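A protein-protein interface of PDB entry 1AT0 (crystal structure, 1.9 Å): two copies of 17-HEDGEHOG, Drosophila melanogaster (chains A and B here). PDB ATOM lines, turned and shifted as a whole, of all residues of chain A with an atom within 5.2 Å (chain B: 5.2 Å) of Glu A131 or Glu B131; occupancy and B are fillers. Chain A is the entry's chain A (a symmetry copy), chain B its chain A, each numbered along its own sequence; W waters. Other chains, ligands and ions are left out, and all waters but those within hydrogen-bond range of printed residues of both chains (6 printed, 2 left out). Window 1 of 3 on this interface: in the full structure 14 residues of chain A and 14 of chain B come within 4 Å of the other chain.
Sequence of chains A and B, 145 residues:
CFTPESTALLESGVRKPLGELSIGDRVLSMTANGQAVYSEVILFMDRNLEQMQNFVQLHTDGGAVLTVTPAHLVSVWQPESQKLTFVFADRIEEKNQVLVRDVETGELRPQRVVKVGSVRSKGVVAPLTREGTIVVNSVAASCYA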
ATOM      1  N   SER A  29       5.330 -16.120 -19.875  1.00  0.00           N
ATOM      2  CA  SER A  29       5.471 -15.051 -20.848  1.00  0.00           C
ATOM      3  C   SER A  29       6.303 -15.559 -22.014  1.00  0.00           C
ATOM      4  O   SER A  29       6.586 -16.753 -22.102  1.00  0.00           O
ATOM      5  CB  SER A  29       6.149 -13.844 -20.194  1.00  0.00           C
ATOM      6  OG  SER A  29       5.347 -13.349 -19.135  1.00  0.00           O
ATOM      7  N   MET A  30       6.699 -14.648 -22.899  1.00  0.00           N
ATOM      8  CA  MET A  30       7.487 -14.998 -24.078  1.00  0.00           C
ATOM      9  C   MET A  30       8.636 -14.015 -24.284  1.00  0.00           C
ATOM     10  O   MET A  30       8.460 -12.805 -24.154  1.00  0.00           O
ATOM     11  CB  MET A  30       6.584 -14.990 -25.314  1.00  0.00           C
ATOM     12  CG  MET A  30       7.278 -15.408 -26.594  1.00  0.00           C
ATOM     13  SD  MET A  30       6.169 -15.062 -28.145  1.00  0.00           S
ATOM     14  CE  MET A  30       6.385 -13.160 -28.220  1.00  0.00           C
ATOM     15  N   THR A  31       9.814 -14.537 -24.593  1.00  0.00           N
ATOM     16  CA  THR A  31      10.971 -13.689 -24.828  1.00  0.00           C
ATOM     17  C   THR A  31      10.858 -13.084 -26.227  1.00  0.00           C
ATOM     18  O   THR A  31      10.000 -13.487 -27.016  1.00  0.00           O
ATOM     19  CB  THR A  31      12.283 -14.492 -24.726  1.00  0.00           C
ATOM     20  OG1 THR A  31      12.285 -15.535 -25.707  1.00  0.00           O
ATOM     21  CG2 THR A  31      12.418 -15.108 -23.350  1.00  0.00           C
ATOM     22  N   ALA A  32      11.747 -12.149 -26.547  1.00  0.00           N
ATOM     23  CA  ALA A  32      11.738 -11.497 -27.851  1.00  0.00           C
ATOM     24  C   ALA A  32      11.888 -12.509 -28.980  1.00  0.00           C
ATOM     25  O   ALA A  32      11.364 -12.301 -30.073  1.00  0.00           O
ATOM     26  CB  ALA A  32      12.833 -10.449 -27.931  1.00  0.00           C
ATOM     27  N   VAL A  37       9.090 -18.234 -20.865  1.00  0.00           N
ATOM     28  CA  VAL A  37       9.848 -17.732 -19.723  1.00  0.00           C
ATOM     29  C   VAL A  37       8.842 -17.195 -18.712  1.00  0.00           C
ATOM     30  O   VAL A  37       7.741 -16.811 -19.087  1.00  0.00           O
ATOM     31  CB  VAL A  37      10.817 -16.601 -20.142  1.00  0.00           C
ATOM     32  CG1 VAL A  37      10.051 -15.411 -20.691  1.00  0.00           C
ATOM     33  CG2 VAL A  37      11.676 -16.182 -18.968  1.00  0.00           C
ATOM     34  N   SER A  39       7.706 -14.406 -15.932  1.00  0.00           N
ATOM     35  CA  SER A  39       7.960 -13.004 -15.624  1.00  0.00           C
ATOM     36  C   SER A  39       6.906 -12.505 -14.642  1.00  0.00           C
ATOM     37  O   SER A  39       5.758 -12.945 -14.688  1.00  0.00           O
ATOM     38  CB  SER A  39       7.892 -12.185 -16.923  1.00  0.00           C
ATOM     39  OG  SER A  39       8.325 -10.846 -16.738  1.00  0.00           O
ATOM     40  N   THR A 129       3.678  -7.507 -17.638  1.00  0.00           N
ATOM     41  CA  THR A 129       4.768  -8.255 -17.008  1.00  0.00           C
ATOM     42  C   THR A 129       6.102  -7.550 -17.293  1.00  0.00           C
ATOM     43  O   THR A 129       6.154  -6.644 -18.133  1.00  0.00           O
ATOM     44  CB  THR A 129       4.842  -9.680 -17.590  1.00  0.00           C
ATOM     45  OG1 THR A 129       5.132  -9.605 -18.994  1.00  0.00           O
ATOM     46  CG2 THR A 129       3.519 -10.411 -17.394  1.00  0.00           C
ATOM     47  N   ARG A 130       7.178  -7.963 -16.621  1.00  0.00           N
ATOM     48  CA  ARG A 130       8.491  -7.361 -16.871  1.00  0.00           C
ATOM     49  C   ARG A 130       8.943  -7.616 -18.300  1.00  0.00           C
ATOM     50  O   ARG A 130       9.595  -6.773 -18.909  1.00  0.00           O
ATOM     51  CB  ARG A 130       9.555  -7.914 -15.930  1.00  0.00           C
ATOM     52  CG  ARG A 130       9.507  -7.349 -14.543  1.00  0.00           C
ATOM     53  CD  ARG A 130      10.723  -7.779 -13.739  1.00  0.00           C
ATOM     54  NE  ARG A 130      10.611  -7.261 -12.389  1.00  0.00           N
ATOM     55  CZ  ARG A 130      11.143  -6.116 -11.976  1.00  0.00           C
ATOM     56  NH1 ARG A 130      11.857  -5.365 -12.810  1.00  0.00           N
ATOM     57  NH2 ARG A 130      10.850  -5.662 -10.762  1.00  0.00           N
ATOM     58  N   GLU A 131       8.612  -8.796 -18.818  1.00  0.00           N
ATOM     59  CA  GLU A 131       8.970  -9.176 -20.181  1.00  0.00           C
ATOM     60  C   GLU A 131       8.202  -8.374 -21.219  1.00  0.00           C
ATOM     61  O   GLU A 131       8.705  -8.131 -22.316  1.00  0.00           O
ATOM     62  CB  GLU A 131       8.724 -10.671 -20.403  1.00  0.00           C
ATOM     63  CG  GLU A 131       9.864 -11.559 -19.935  1.00  0.00           C
ATOM     64  CD  GLU A 131      11.165 -11.284 -20.673  1.00  0.00           C
ATOM     65  OE1 GLU A 131      11.164 -11.273 -21.923  1.00  0.00           O
ATOM     66  OE2 GLU A 131      12.198 -11.085 -20.005  1.00  0.00           O
ATOM     67  N   GLY A 132       6.977  -7.983 -20.875  1.00  0.00           N
ATOM     68  CA  GLY A 132       6.157  -7.208 -21.787  1.00  0.00           C
ATOM     69  C   GLY A 132       5.213  -8.081 -22.590  1.00  0.00           C
ATOM     70  O   GLY A 132       4.421  -7.586 -23.393  1.00  0.00           O
ATOM     71  N   THR A 133       5.295  -9.387 -22.374  1.00  0.00           N
ATOM     72  CA  THR A 133       4.442 -10.343 -23.068  1.00  0.00           C
ATOM     73  C   THR A 133       3.783 -11.240 -22.027  1.00  0.00           C
ATOM     74  O   THR A 133       4.206 -11.274 -20.864  1.00  0.00           O
ATOM     75  CB  THR A 133       5.262 -11.238 -24.008  1.00  0.00           C
ATOM     76  OG1 THR A 133       6.324 -11.839 -23.263  1.00  0.00           O
ATOM     77  CG2 THR A 133       5.853 -10.430 -25.159  1.00  0.00           C
ATOM     78  N   SER B  29      17.872  -1.113 -25.920  1.00  0.00           N
ATOM     79  CA  SER B  29      16.806  -1.424 -24.984  1.00  0.00           C
ATOM     80  C   SER B  29      17.408  -2.092 -23.760  1.00  0.00           C
ATOM     81  O   SER B  29      18.629  -2.130 -23.611  1.00  0.00           O
ATOM     82  CB  SER B  29      15.787  -2.352 -25.652  1.00  0.00           C
ATOM     83  OG  SER B  29      15.197  -1.706 -26.768  1.00  0.00           O
ATOM     84  N   MET B  30      16.551  -2.624 -22.894  1.00  0.00           N
ATOM     85  CA  MET B  30      16.990  -3.280 -21.665  1.00  0.00           C
ATOM     86  C   MET B  30      16.242  -4.591 -21.443  1.00  0.00           C
ATOM     87  O   MET B  30      15.029  -4.663 -21.629  1.00  0.00           O
ATOM     88  CB  MET B  30      16.746  -2.348 -20.476  1.00  0.00           C
ATOM     89  CG  MET B  30      17.229  -2.894 -19.148  1.00  0.00           C
ATOM     90  SD  MET B  30      16.598  -1.815 -17.668  1.00  0.00           S
ATOM     91  CE  MET B  30      14.773  -2.398 -17.658  1.00  0.00           C
ATOM     92  N   THR B  31      16.968  -5.630 -21.057  1.00  0.00           N
ATOM     93  CA  THR B  31      16.353  -6.921 -20.799  1.00  0.00           C
ATOM     94  C   THR B  31      15.669  -6.874 -19.432  1.00  0.00           C
ATOM     95  O   THR B  31      15.858  -5.923 -18.671  1.00  0.00           O
ATOM     96  CB  THR B  31      17.400  -8.052 -20.805  1.00  0.00           C
ATOM     97  OG1 THR B  31      18.375  -7.808 -19.785  1.00  0.00           O
ATOM     98  CG2 THR B  31      18.097  -8.117 -22.147  1.00  0.00           C
ATOM     99  N   ALA B  32      14.912  -7.917 -19.108  1.00  0.00           N
ATOM    100  CA  ALA B  32      14.208  -7.984 -17.832  1.00  0.00           C
ATOM    101  C   ALA B  32      15.174  -7.887 -16.658  1.00  0.00           C
ATOM    102  O   ALA B  32      14.814  -7.371 -15.600  1.00  0.00           O
ATOM    103  CB  ALA B  32      13.391  -9.261 -17.741  1.00  0.00           C
ATOM    104  N   VAL B  37      20.629  -4.339 -24.664  1.00  0.00           N
ATOM    105  CA  VAL B  37      20.341  -5.226 -25.787  1.00  0.00           C
ATOM    106  C   VAL B  37      19.668  -4.387 -26.867  1.00  0.00           C
ATOM    107  O   VAL B  37      19.058  -3.370 -26.562  1.00  0.00           O
ATOM    108  CB  VAL B  37      19.403  -6.382 -25.367  1.00  0.00           C
ATOM    109  CG1 VAL B  37      18.060  -5.845 -24.904  1.00  0.00           C
ATOM    110  CG2 VAL B  37      19.217  -7.353 -26.514  1.00  0.00           C
ATOM    111  N   SER B  39      16.849  -3.936 -29.808  1.00  0.00           N
ATOM    112  CA  SER B  39      15.540  -4.474 -30.158  1.00  0.00           C
ATOM    113  C   SER B  39      14.893  -3.579 -31.210  1.00  0.00           C
ATOM    114  O   SER B  39      15.098  -2.366 -31.203  1.00  0.00           O
ATOM    115  CB  SER B  39      14.662  -4.517 -28.898  1.00  0.00           C
ATOM    116  OG  SER B  39      13.444  -5.213 -29.115  1.00  0.00           O
ATOM    117  N   THR B 129       9.221  -1.284 -28.576  1.00  0.00           N
ATOM    118  CA  THR B 129      10.198  -2.230 -29.122  1.00  0.00           C
ATOM    119  C   THR B 129       9.754  -3.665 -28.801  1.00  0.00           C
ATOM    120  O   THR B 129       8.836  -3.861 -27.996  1.00  0.00           O
ATOM    121  CB  THR B 129      11.579  -1.997 -28.480  1.00  0.00           C
ATOM    122  OG1 THR B 129      11.495  -2.241 -27.068  1.00  0.00           O
ATOM    123  CG2 THR B 129      12.047  -0.566 -28.712  1.00  0.00           C
ATOM    124  N   ARG B 130      10.402  -4.663 -29.403  1.00  0.00           N
ATOM    125  CA  ARG B 130      10.057  -6.058 -29.114  1.00  0.00           C
ATOM    126  C   ARG B 130      10.325  -6.393 -27.655  1.00  0.00           C
ATOM    127  O   ARG B 130       9.597  -7.175 -27.049  1.00  0.00           O
ATOM    128  CB  ARG B 130      10.852  -7.029 -29.978  1.00  0.00           C
ATOM    129  CG  ARG B 130      10.356  -7.149 -31.388  1.00  0.00           C
ATOM    130  CD  ARG B 130      11.055  -8.287 -32.114  1.00  0.00           C
ATOM    131  NE  ARG B 130      10.591  -8.334 -33.488  1.00  0.00           N
ATOM    132  CZ  ARG B 130       9.594  -9.097 -33.919  1.00  0.00           C
ATOM    133  NH1 ARG B 130       8.957  -9.912 -33.082  1.00  0.00           N
ATOM    134  NH2 ARG B 130       9.151  -8.948 -35.163  1.00  0.00           N
ATOM    135  N   GLU B 131      11.391  -5.816 -27.107  1.00  0.00           N
ATOM    136  CA  GLU B 131      11.767  -6.037 -25.714  1.00  0.00           C
ATOM    137  C   GLU B 131      10.780  -5.402 -24.748  1.00  0.00           C
ATOM    138  O   GLU B 131      10.587  -5.899 -23.638  1.00  0.00           O
ATOM    139  CB  GLU B 131      13.172  -5.493 -25.445  1.00  0.00           C
ATOM    140  CG  GLU B 131      14.288  -6.453 -25.821  1.00  0.00           C
ATOM    141  CD  GLU B 131      14.237  -7.752 -25.032  1.00  0.00           C
ATOM    142  OE1 GLU B 131      14.165  -7.703 -23.785  1.00  0.00           O
ATOM    143  OE2 GLU B 131      14.276  -8.829 -25.657  1.00  0.00           O
ATOM    144  N   GLY B 132      10.175  -4.293 -25.166  1.00  0.00           N
ATOM    145  CA  GLY B 132       9.211  -3.606 -24.326  1.00  0.00           C
ATOM    146  C   GLY B 132       9.843  -2.478 -23.536  1.00  0.00           C
ATOM    147  O   GLY B 132       9.164  -1.767 -22.793  1.00  0.00           O
ATOM    148  N   THR B 133      11.148  -2.308 -23.696  1.00  0.00           N
ATOM    149  CA  THR B 133      11.885  -1.257 -23.006  1.00  0.00           C
ATOM    150  C   THR B 133      12.685  -0.475 -24.042  1.00  0.00           C
ATOM    151  O   THR B 133      12.858  -0.930 -25.180  1.00  0.00           O
ATOM    152  CB  THR B 133      12.875  -1.846 -21.993  1.00  0.00           C
ATOM    153  OG1 THR B 133      13.709  -2.797 -22.660  1.00  0.00           O
ATOM    154  CG2 THR B 133      12.143  -2.539 -20.848  1.00  0.00           C
HETATM  155  O   HOH W   1      12.859 -11.044 -24.372  1.00  0.00           O
HETATM  156  O   HOH W   2      14.153  -9.311 -21.268  1.00  0.00           O
HETATM  157  O   HOH W   3      10.837  -9.123 -24.014  1.00  0.00           O
HETATM  158  O   HOH W   4       8.856 -10.834 -30.588  1.00  0.00           O
HETATM  159  O   HOH W   5      12.863  -5.183 -15.268  1.00  0.00           O
HETATM  160  O   HOH W   6      11.893  -7.723 -21.800  1.00  0.00           O
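The backbone NH of Glu B131 lies within hydrogen-bond range of the side-chain hydroxyl of Ser B39 (2.9 Å).
OG of Ser A39 sits at hydrogen-bond distance from N of Glu A131 (2.9 Å).
The backbone carbonyl oxygen (O) of Glu A131 lies close to the backbone carbonyl oxygen (O) of Glu B131 (3.2 Å).
Of the printed residues of chain B, Ala A32 touches Glu B131.
Of the printed residues of chain A, Ala B32 touches Glu A131 (3.1 Å).
Thr B129 touches none of the printed residues of chain A.
Arg B130 touches none of the printed residues of chain A.
Glu B131 touches just these residues of chain A: Ala A32 (3.1 Å) and Glu A131 (3.2 Å).
The nearest residue of chain A that does not touch Glu B131 is Arg A130 (4.9 Å).
Of the 11 printed residues of chain B, 2 touch a printed residue of chain A.
Hydrophobic or aromatic side chains of chain B within 4 Å of the printed part of chain A: Ala B32.
Printed residues of chain A that touch a printed residue of chain B: Ala A32 and Glu A131.
Among the printed residues, 3 pairs touch across the chains.
Ala A32 touches Glu B131, and with the chains exchanged Glu A131 touches Ala B32.
Glu B131 touches its own counterpart, Glu A131.
11 positions are printed for both chains.
Water W5 bridges the guanidinium group (NH1) of Arg A130 (2.7 Å) and the backbone carbonyl oxygen (O) of Ala B32 (3.0 Å).
Water W4 bridges the guanidinium group (NH1) of Arg B130 (2.7 Å) and the backbone carbonyl oxygen (O) of Ala A32 (3.0 Å).
Water W2 lies within hydrogen-bond range of the backbone NH of Ala B32 (2.7 Å), the side-chain carboxylate of Glu A131 (2.9 Å) and the side-chain carboxylate of Glu B131 (3.0 Å).
Water W1 lies within hydrogen-bond range of N of Ala A32 (2.7 Å), OE2 of Glu B131 (2.9 Å) and OE1 of Glu A131 (3.0 Å).
Water W3 lies within hydrogen-bond range of the backbone carbonyl oxygen of Glu A131 (2.9 Å) and the backbone carbonyl oxygen of Glu B131 (3.3 Å).
Water W6 lies within hydrogen-bond range of the backbone carbonyl oxygen of Glu B131 (2.9 Å) and the backbone carbonyl oxygen of Glu A131 (3.3 Å).
Among the printed residues, merely in contact across the chains: Ala A32 with Glu B131 and Glu A131 with Ala B32.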
